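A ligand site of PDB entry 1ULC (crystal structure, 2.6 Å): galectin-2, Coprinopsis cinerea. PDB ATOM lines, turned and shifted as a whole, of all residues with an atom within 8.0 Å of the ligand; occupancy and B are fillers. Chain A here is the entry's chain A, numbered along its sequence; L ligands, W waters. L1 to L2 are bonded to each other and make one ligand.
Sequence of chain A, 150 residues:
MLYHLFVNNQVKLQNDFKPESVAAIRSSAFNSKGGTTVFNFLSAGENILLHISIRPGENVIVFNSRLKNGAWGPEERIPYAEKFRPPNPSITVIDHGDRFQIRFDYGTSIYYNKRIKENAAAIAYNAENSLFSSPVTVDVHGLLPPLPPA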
ATOM      1  N   THR A  36     -26.977   9.635 -20.341  1.00  0.00           N
ATOM      2  CA  THR A  36     -26.599  11.036 -20.432  1.00  0.00           C
ATOM      3  C   THR A  36     -27.803  11.939 -20.642  1.00  0.00           C
ATOM      4  O   THR A  36     -28.613  11.724 -21.554  1.00  0.00           O
ATOM      5  CB  THR A  36     -25.571  11.248 -21.546  1.00  0.00           C
ATOM      6  OG1 THR A  36     -24.338  10.632 -21.146  1.00  0.00           O
ATOM      7  CG2 THR A  36     -25.329  12.726 -21.798  1.00  0.00           C
ATOM      8  N   VAL A  38     -28.937  16.038 -20.954  1.00  0.00           N
ATOM      9  CA  VAL A  38     -28.439  17.370 -21.262  1.00  0.00           C
ATOM     10  C   VAL A  38     -29.447  18.496 -21.089  1.00  0.00           C
ATOM     11  O   VAL A  38     -30.642  18.316 -21.347  1.00  0.00           O
ATOM     12  CB  VAL A  38     -27.900  17.417 -22.721  1.00  0.00           C
ATOM     13  CG1 VAL A  38     -27.594  18.843 -23.125  1.00  0.00           C
ATOM     14  CG2 VAL A  38     -26.657  16.559 -22.833  1.00  0.00           C
ATOM     15  N   ASN A  40     -29.512  22.679 -22.045  1.00  0.00           N
ATOM     16  CA  ASN A  40     -28.844  23.819 -22.680  1.00  0.00           C
ATOM     17  C   ASN A  40     -29.580  25.129 -22.477  1.00  0.00           C
ATOM     18  O   ASN A  40     -30.807  25.175 -22.541  1.00  0.00           O
ATOM     19  CB  ASN A  40     -28.734  23.622 -24.201  1.00  0.00           C
ATOM     20  CG  ASN A  40     -27.822  22.489 -24.580  1.00  0.00           C
ATOM     21  OD1 ASN A  40     -26.721  22.351 -24.061  1.00  0.00           O
ATOM     22  ND2 ASN A  40     -28.280  21.670 -25.517  1.00  0.00           N
ATOM     23  N   HIS A  51     -23.952  24.773 -21.502  1.00  0.00           N
ATOM     24  CA  HIS A  51     -24.241  23.372 -21.812  1.00  0.00           C
ATOM     25  C   HIS A  51     -23.906  22.539 -20.581  1.00  0.00           C
ATOM     26  O   HIS A  51     -22.788  22.623 -20.050  1.00  0.00           O
ATOM     27  CB  HIS A  51     -23.384  22.897 -22.999  1.00  0.00           C
ATOM     28  CG  HIS A  51     -23.472  21.417 -23.290  1.00  0.00           C
ATOM     29  ND1 HIS A  51     -24.598  20.834 -23.828  1.00  0.00           N
ATOM     30  CD2 HIS A  51     -22.567  20.428 -23.133  1.00  0.00           C
ATOM     31  CE1 HIS A  51     -24.375  19.536 -23.992  1.00  0.00           C
ATOM     32  NE2 HIS A  51     -23.161  19.264 -23.578  1.00  0.00           N
ATOM     33  N   ILE A  52     -24.871  21.757 -20.123  1.00  0.00           N
ATOM     34  CA  ILE A  52     -24.680  20.892 -18.974  1.00  0.00           C
ATOM     35  C   ILE A  52     -24.916  19.463 -19.448  1.00  0.00           C
ATOM     36  O   ILE A  52     -26.007  19.101 -19.875  1.00  0.00           O
ATOM     37  CB  ILE A  52     -25.676  21.185 -17.832  1.00  0.00           C
ATOM     38  CG1 ILE A  52     -25.699  22.684 -17.525  1.00  0.00           C
ATOM     39  CG2 ILE A  52     -25.268  20.438 -16.582  1.00  0.00           C
ATOM     40  CD1 ILE A  52     -26.701  23.078 -16.429  1.00  0.00           C
ATOM     41  N   SER A  53     -23.865  18.654 -19.385  1.00  0.00           N
ATOM     42  CA  SER A  53     -23.947  17.274 -19.816  1.00  0.00           C
ATOM     43  C   SER A  53     -23.760  16.392 -18.583  1.00  0.00           C
ATOM     44  O   SER A  53     -22.654  16.272 -18.051  1.00  0.00           O
ATOM     45  CB  SER A  53     -22.877  16.971 -20.863  1.00  0.00           C
ATOM     46  OG  SER A  53     -23.010  15.660 -21.379  1.00  0.00           O
ATOM     47  N   ILE A  54     -24.857  15.798 -18.129  1.00  0.00           N
ATOM     48  CA  ILE A  54     -24.859  14.913 -16.967  1.00  0.00           C
ATOM     49  C   ILE A  54     -24.617  13.475 -17.443  1.00  0.00           C
ATOM     50  O   ILE A  54     -25.514  12.829 -17.989  1.00  0.00           O
ATOM     51  CB  ILE A  54     -26.202  15.011 -16.234  1.00  0.00           C
ATOM     52  CG1 ILE A  54     -26.516  16.472 -15.961  1.00  0.00           C
ATOM     53  CG2 ILE A  54     -26.153  14.231 -14.937  1.00  0.00           C
ATOM     54  CD1 ILE A  54     -27.935  16.704 -15.528  1.00  0.00           C
ATOM     55  N   ARG A  55     -23.402  12.991 -17.234  1.00  0.00           N
ATOM     56  CA  ARG A  55     -23.026  11.654 -17.668  1.00  0.00           C
ATOM     57  C   ARG A  55     -22.874  10.685 -16.504  1.00  0.00           C
ATOM     58  O   ARG A  55     -21.831  10.634 -15.854  1.00  0.00           O
ATOM     59  CB  ARG A  55     -21.726  11.723 -18.457  1.00  0.00           C
ATOM     60  CG  ARG A  55     -21.755  12.782 -19.524  1.00  0.00           C
ATOM     61  CD  ARG A  55     -20.386  13.049 -20.096  1.00  0.00           C
ATOM     62  NE  ARG A  55     -20.453  14.072 -21.134  1.00  0.00           N
ATOM     63  CZ  ARG A  55     -19.429  14.455 -21.890  1.00  0.00           C
ATOM     64  NH1 ARG A  55     -18.238  13.889 -21.733  1.00  0.00           N
ATOM     65  NH2 ARG A  55     -19.606  15.392 -22.800  1.00  0.00           N
ATOM     66  N   GLU A  58     -20.172   7.750 -16.870  1.00  0.00           N
ATOM     67  CA  GLU A  58     -18.797   8.214 -17.061  1.00  0.00           C
ATOM     68  C   GLU A  58     -18.462   8.929 -15.760  1.00  0.00           C
ATOM     69  O   GLU A  58     -17.363   9.442 -15.573  1.00  0.00           O
ATOM     70  CB  GLU A  58     -18.799   9.185 -18.251  1.00  0.00           C
ATOM     71  CG  GLU A  58     -17.502   9.353 -19.028  1.00  0.00           C
ATOM     72  CD  GLU A  58     -17.694  10.266 -20.264  1.00  0.00           C
ATOM     73  OE1 GLU A  58     -18.614  10.002 -21.077  1.00  0.00           O
ATOM     74  OE2 GLU A  58     -16.908  11.236 -20.428  1.00  0.00           O
ATOM     75  N   VAL A  60     -19.430  11.817 -14.482  1.00  0.00           N
ATOM     76  CA  VAL A  60     -18.985  13.187 -14.624  1.00  0.00           C
ATOM     77  C   VAL A  60     -20.084  14.065 -15.215  1.00  0.00           C
ATOM     78  O   VAL A  60     -20.953  13.589 -15.949  1.00  0.00           O
ATOM     79  CB  VAL A  60     -17.715  13.266 -15.514  1.00  0.00           C
ATOM     80  CG1 VAL A  60     -18.063  12.898 -16.962  1.00  0.00           C
ATOM     81  CG2 VAL A  60     -17.119  14.658 -15.434  1.00  0.00           C
ATOM     82  N   VAL A  62     -20.379  17.510 -17.425  1.00  0.00           N
ATOM     83  CA  VAL A  62     -19.545  18.389 -18.240  1.00  0.00           C
ATOM     84  C   VAL A  62     -20.218  19.709 -18.589  1.00  0.00           C
ATOM     85  O   VAL A  62     -21.372  19.732 -18.989  1.00  0.00           O
ATOM     86  CB  VAL A  62     -19.130  17.704 -19.557  1.00  0.00           C
ATOM     87  CG1 VAL A  62     -18.112  18.553 -20.293  1.00  0.00           C
ATOM     88  CG2 VAL A  62     -18.577  16.318 -19.277  1.00  0.00           C
ATOM     89  N   PHE A  63     -19.474  20.799 -18.442  1.00  0.00           N
ATOM     90  CA  PHE A  63     -19.989  22.128 -18.749  1.00  0.00           C
ATOM     91  C   PHE A  63     -19.214  22.697 -19.933  1.00  0.00           C
ATOM     92  O   PHE A  63     -17.995  22.603 -19.984  1.00  0.00           O
ATOM     93  CB  PHE A  63     -19.843  23.083 -17.550  1.00  0.00           C
ATOM     94  CG  PHE A  63     -20.640  22.666 -16.354  1.00  0.00           C
ATOM     95  CD1 PHE A  63     -20.166  21.682 -15.492  1.00  0.00           C
ATOM     96  CD2 PHE A  63     -21.887  23.228 -16.096  1.00  0.00           C
ATOM     97  CE1 PHE A  63     -20.915  21.263 -14.389  1.00  0.00           C
ATOM     98  CE2 PHE A  63     -22.650  22.819 -14.994  1.00  0.00           C
ATOM     99  CZ  PHE A  63     -22.160  21.837 -14.144  1.00  0.00           C
ATOM    100  N   ASN A  64     -19.939  23.275 -20.887  1.00  0.00           N
ATOM    101  CA  ASN A  64     -19.308  23.846 -22.073  1.00  0.00           C
ATOM    102  C   ASN A  64     -20.243  24.843 -22.759  1.00  0.00           C
ATOM    103  O   ASN A  64     -21.379  25.052 -22.335  1.00  0.00           O
ATOM    104  CB  ASN A  64     -18.929  22.736 -23.057  1.00  0.00           C
ATOM    105  CG  ASN A  64     -17.635  23.042 -23.814  1.00  0.00           C
ATOM    106  OD1 ASN A  64     -17.275  24.197 -23.996  1.00  0.00           O
ATOM    107  ND2 ASN A  64     -16.948  21.990 -24.270  1.00  0.00           N
ATOM    108  N   SER A  65     -19.734  25.463 -23.828  1.00  0.00           N
ATOM    109  CA  SER A  65     -20.469  26.446 -24.613  1.00  0.00           C
ATOM    110  C   SER A  65     -20.036  26.301 -26.069  1.00  0.00           C
ATOM    111  O   SER A  65     -18.989  25.716 -26.345  1.00  0.00           O
ATOM    112  CB  SER A  65     -20.144  27.876 -24.149  1.00  0.00           C
ATOM    113  OG  SER A  65     -20.505  28.116 -22.807  1.00  0.00           O
ATOM    114  N   ARG A  66     -20.829  26.842 -26.986  1.00  0.00           N
ATOM    115  CA  ARG A  66     -20.483  26.833 -28.403  1.00  0.00           C
ATOM    116  C   ARG A  66     -21.543  27.605 -29.176  1.00  0.00           C
ATOM    117  O   ARG A  66     -22.700  27.645 -28.776  1.00  0.00           O
ATOM    118  CB  ARG A  66     -20.340  25.403 -28.957  1.00  0.00           C
ATOM    119  CG  ARG A  66     -21.627  24.736 -29.371  1.00  0.00           C
ATOM    120  CD  ARG A  66     -21.358  23.352 -29.963  1.00  0.00           C
ATOM    121  NE  ARG A  66     -22.579  22.744 -30.468  1.00  0.00           N
ATOM    122  CZ  ARG A  66     -23.142  23.016 -31.634  1.00  0.00           C
ATOM    123  NH1 ARG A  66     -22.588  23.901 -32.455  1.00  0.00           N
ATOM    124  NH2 ARG A  66     -24.260  22.427 -31.995  1.00  0.00           N
ATOM    125  N   ALA A  71     -17.505  25.198 -32.856  1.00  0.00           N
ATOM    126  CA  ALA A  71     -16.995  24.033 -32.156  1.00  0.00           C
ATOM    127  C   ALA A  71     -17.108  24.245 -30.655  1.00  0.00           C
ATOM    128  O   ALA A  71     -17.303  25.366 -30.181  1.00  0.00           O
ATOM    129  CB  ALA A  71     -15.552  23.789 -32.535  1.00  0.00           C
ATOM    130  N   TRP A  72     -17.008  23.140 -29.913  1.00  0.00           N
ATOM    131  CA  TRP A  72     -17.070  23.187 -28.457  1.00  0.00           C
ATOM    132  C   TRP A  72     -15.785  23.819 -27.977  1.00  0.00           C
ATOM    133  O   TRP A  72     -14.776  23.803 -28.677  1.00  0.00           O
ATOM    134  CB  TRP A  72     -17.167  21.780 -27.871  1.00  0.00           C
ATOM    135  CG  TRP A  72     -18.477  21.096 -28.102  1.00  0.00           C
ATOM    136  CD1 TRP A  72     -18.709  20.006 -28.882  1.00  0.00           C
ATOM    137  CD2 TRP A  72     -19.734  21.445 -27.506  1.00  0.00           C
ATOM    138  NE1 TRP A  72     -20.032  19.638 -28.815  1.00  0.00           N
ATOM    139  CE2 TRP A  72     -20.678  20.507 -27.974  1.00  0.00           C
ATOM    140  CE3 TRP A  72     -20.142  22.444 -26.624  1.00  0.00           C
ATOM    141  CZ2 TRP A  72     -22.029  20.542 -27.581  1.00  0.00           C
ATOM    142  CZ3 TRP A  72     -21.479  22.479 -26.228  1.00  0.00           C
ATOM    143  CH2 TRP A  72     -22.398  21.534 -26.714  1.00  0.00           C
ATOM    144  N   GLY A  73     -15.822  24.389 -26.778  1.00  0.00           N
ATOM    145  CA  GLY A  73     -14.630  24.984 -26.207  1.00  0.00           C
ATOM    146  C   GLY A  73     -14.044  23.994 -25.227  1.00  0.00           C
ATOM    147  O   GLY A  73     -14.292  22.794 -25.325  1.00  0.00           O
ATOM    148  N   PRO A  74     -13.234  24.456 -24.272  1.00  0.00           N
ATOM    149  CA  PRO A  74     -12.690  23.476 -23.336  1.00  0.00           C
ATOM    150  C   PRO A  74     -13.755  23.030 -22.322  1.00  0.00           C
ATOM    151  O   PRO A  74     -14.607  23.828 -21.909  1.00  0.00           O
ATOM    152  CB  PRO A  74     -11.509  24.221 -22.700  1.00  0.00           C
ATOM    153  CG  PRO A  74     -11.923  25.667 -22.791  1.00  0.00           C
ATOM    154  CD  PRO A  74     -12.566  25.757 -24.151  1.00  0.00           C
ATOM    155  N   GLU A  75     -13.730  21.754 -21.934  1.00  0.00           N
ATOM    156  CA  GLU A  75     -14.713  21.239 -20.990  1.00  0.00           C
ATOM    157  C   GLU A  75     -14.342  21.495 -19.544  1.00  0.00           C
ATOM    158  O   GLU A  75     -13.185  21.373 -19.157  1.00  0.00           O
ATOM    159  CB  GLU A  75     -14.892  19.727 -21.166  1.00  0.00           C
ATOM    160  CG  GLU A  75     -15.356  19.292 -22.527  1.00  0.00           C
ATOM    161  CD  GLU A  75     -15.709  17.818 -22.579  1.00  0.00           C
ATOM    162  OE1 GLU A  75     -15.140  17.048 -21.771  1.00  0.00           O
ATOM    163  OE2 GLU A  75     -16.535  17.428 -23.434  1.00  0.00           O
ATOM    164  N   GLU A  76     -15.353  21.863 -18.766  1.00  0.00           N
ATOM    165  CA  GLU A  76     -15.190  22.085 -17.336  1.00  0.00           C
ATOM    166  C   GLU A  76     -16.010  20.944 -16.735  1.00  0.00           C
ATOM    167  O   GLU A  76     -17.226  20.864 -16.933  1.00  0.00           O
ATOM    168  CB  GLU A  76     -15.720  23.475 -16.947  1.00  0.00           C
ATOM    169  CG  GLU A  76     -14.796  24.592 -17.391  1.00  0.00           C
ATOM    170  CD  GLU A  76     -15.265  25.986 -16.981  1.00  0.00           C
ATOM    171  OE1 GLU A  76     -15.678  26.172 -15.822  1.00  0.00           O
ATOM    172  OE2 GLU A  76     -15.204  26.895 -17.823  1.00  0.00           O
ATOM    173  N   ARG A  77     -15.334  20.049 -16.026  1.00  0.00           N
ATOM    174  CA  ARG A  77     -15.978  18.860 -15.455  1.00  0.00           C
ATOM    175  C   ARG A  77     -16.041  18.790 -13.927  1.00  0.00           C
ATOM    176  O   ARG A  77     -15.412  19.575 -13.233  1.00  0.00           O
ATOM    177  CB  ARG A  77     -15.236  17.612 -15.954  1.00  0.00           C
ATOM    178  CG  ARG A  77     -15.240  17.411 -17.448  1.00  0.00           C
ATOM    179  CD  ARG A  77     -14.030  16.590 -17.885  1.00  0.00           C
ATOM    180  NE  ARG A  77     -14.206  16.011 -19.213  1.00  0.00           N
ATOM    181  CZ  ARG A  77     -14.744  14.823 -19.445  1.00  0.00           C
ATOM    182  NH1 ARG A  77     -15.155  14.069 -18.433  1.00  0.00           N
ATOM    183  NH2 ARG A  77     -14.879  14.377 -20.686  1.00  0.00           N
ATOM    184  N   ARG A 115     -19.001  32.774 -21.565  1.00  0.00           N
ATOM    185  CA  ARG A 115     -18.089  32.761 -22.713  1.00  0.00           C
ATOM    186  C   ARG A 115     -18.698  33.469 -23.910  1.00  0.00           C
ATOM    187  O   ARG A 115     -17.966  33.979 -24.762  1.00  0.00           O
ATOM    188  CB  ARG A 115     -17.751  31.312 -23.096  1.00  0.00           C
ATOM    189  CG  ARG A 115     -17.071  30.509 -21.991  1.00  0.00           C
ATOM    190  CD  ARG A 115     -16.706  29.134 -22.487  1.00  0.00           C
ATOM    191  NE  ARG A 115     -16.123  28.305 -21.445  1.00  0.00           N
ATOM    192  CZ  ARG A 115     -15.669  27.068 -21.628  1.00  0.00           C
ATOM    193  NH1 ARG A 115     -15.735  26.499 -22.819  1.00  0.00           N
ATOM    194  NH2 ARG A 115     -15.160  26.387 -20.601  1.00  0.00           N
HETATM  195  C1  LIG L   1     -14.554  14.304 -24.997  1.00  0.00           C
HETATM  196  C2  LIG L   1     -16.068  14.286 -24.775  1.00  0.00           C
HETATM  197  C3  LIG L   1     -16.761  14.982 -25.956  1.00  0.00           C
HETATM  198  C4  LIG L   1     -16.325  14.351 -27.288  1.00  0.00           C
HETATM  199  C5  LIG L   1     -16.822  15.139 -28.482  1.00  0.00           C
HETATM  200  C6  LIG L   1     -14.270  13.612 -26.315  1.00  0.00           C
HETATM  201  O1  LIG L   1     -12.901  13.594 -26.547  1.00  0.00           O
HETATM  202  O2  LIG L   1     -13.893  13.652 -23.932  1.00  0.00           O
HETATM  203  O3  LIG L   1     -16.392  14.939 -23.562  1.00  0.00           O
HETATM  204  O4  LIG L   1     -18.188  14.854 -25.804  1.00  0.00           O
HETATM  205  O5  LIG L   1     -14.882  14.335 -27.385  1.00  0.00           O
HETATM  206  O6  LIG L   1     -16.369  16.488 -28.427  1.00  0.00           O
HETATM  207  C1  LG2 L   2     -18.960  15.931 -26.202  1.00  0.00           C
HETATM  208  C2  LG2 L   2     -20.425  15.476 -26.242  1.00  0.00           C
HETATM  209  C3  LG2 L   2     -21.362  16.664 -26.469  1.00  0.00           C
HETATM  210  C4  LG2 L   2     -21.068  17.777 -25.456  1.00  0.00           C
HETATM  211  C5  LG2 L   2     -19.590  18.138 -25.506  1.00  0.00           C
HETATM  212  C6  LG2 L   2     -19.233  19.172 -24.467  1.00  0.00           C
HETATM  213  O1  LG2 L   2     -20.589  14.520 -27.283  1.00  0.00           O
HETATM  214  O2  LG2 L   2     -22.714  16.244 -26.345  1.00  0.00           O
HETATM  215  O3  LG2 L   2     -21.411  17.349 -24.150  1.00  0.00           O
HETATM  216  O4  LG2 L   2     -18.783  16.974 -25.236  1.00  0.00           O
HETATM  217  O5  LG2 L   2     -17.872  19.532 -24.549  1.00  0.00           O
HETATM  218  O   HOH W   1     -23.233  14.865 -24.030  1.00  0.00           O
HETATM  219  O   HOH W   2     -12.371  11.101 -27.971  1.00  0.00           O
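The side-chain amide nitrogen of Asn 64 lies within hydrogen-bond range of an oxygen (O5) of LG2 L2.
An oxygen (O3) of LIG L1 sits at hydrogen-bond distance from the guanidinium group (NH2) of Arg 77 (3.3 Å).
The side-chain carboxylate (OE2) of Glu 75 is in hydrogen-bond range of an oxygen (O3) of LIG L1 (2.5 Å).
An oxygen (O3) of LG2 L2 is in hydrogen-bond range of a ring nitrogen (NE2) of His 51 (2.7 Å).
An oxygen (O3) of LIG L1 sits at hydrogen-bond distance from the guanidinium group (NH1) of Arg 55 (2.8 Å).
Merely in contact with the ligand: Ser 53 and Trp 72.
Hydrophobic or aromatic side chains that line the ligand: His 51 and Trp 72.
Water W1 bridges an oxygen (O2) of LG2 L2 and the side-chain hydroxyl of Ser 53.
OE2 of Glu 75 is in salt-bridge range of NH2 of Arg 55 (3.7 Å).
N of Arg 55 lies within hydrogen-bond range of O of Val 60 (2.8 Å).
The side-chain carboxylate (OE2) of Glu 58 is in salt-bridge range of the guanidinium group (NH1) of Arg 55 (3.2 Å).
The side-chain carboxylate (OE2) of Glu 58 lies within salt-bridge range of the guanidinium group (NH2) of Arg 77, 3.7 Å away.
The side-chain carboxylate (OE1) of Glu 75 lies within salt-bridge range of the guanidinium group (NH2) of Arg 77 (2.9 Å).
N of His 51 lies within hydrogen-bond range of O of Asn 64, at 2.7 Å.
ND1 of His 51 sits at hydrogen-bond distance from OD1 of Asn 40.
O of Ser 53 lies within hydrogen-bond range of N of Val 62 (2.7 Å).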
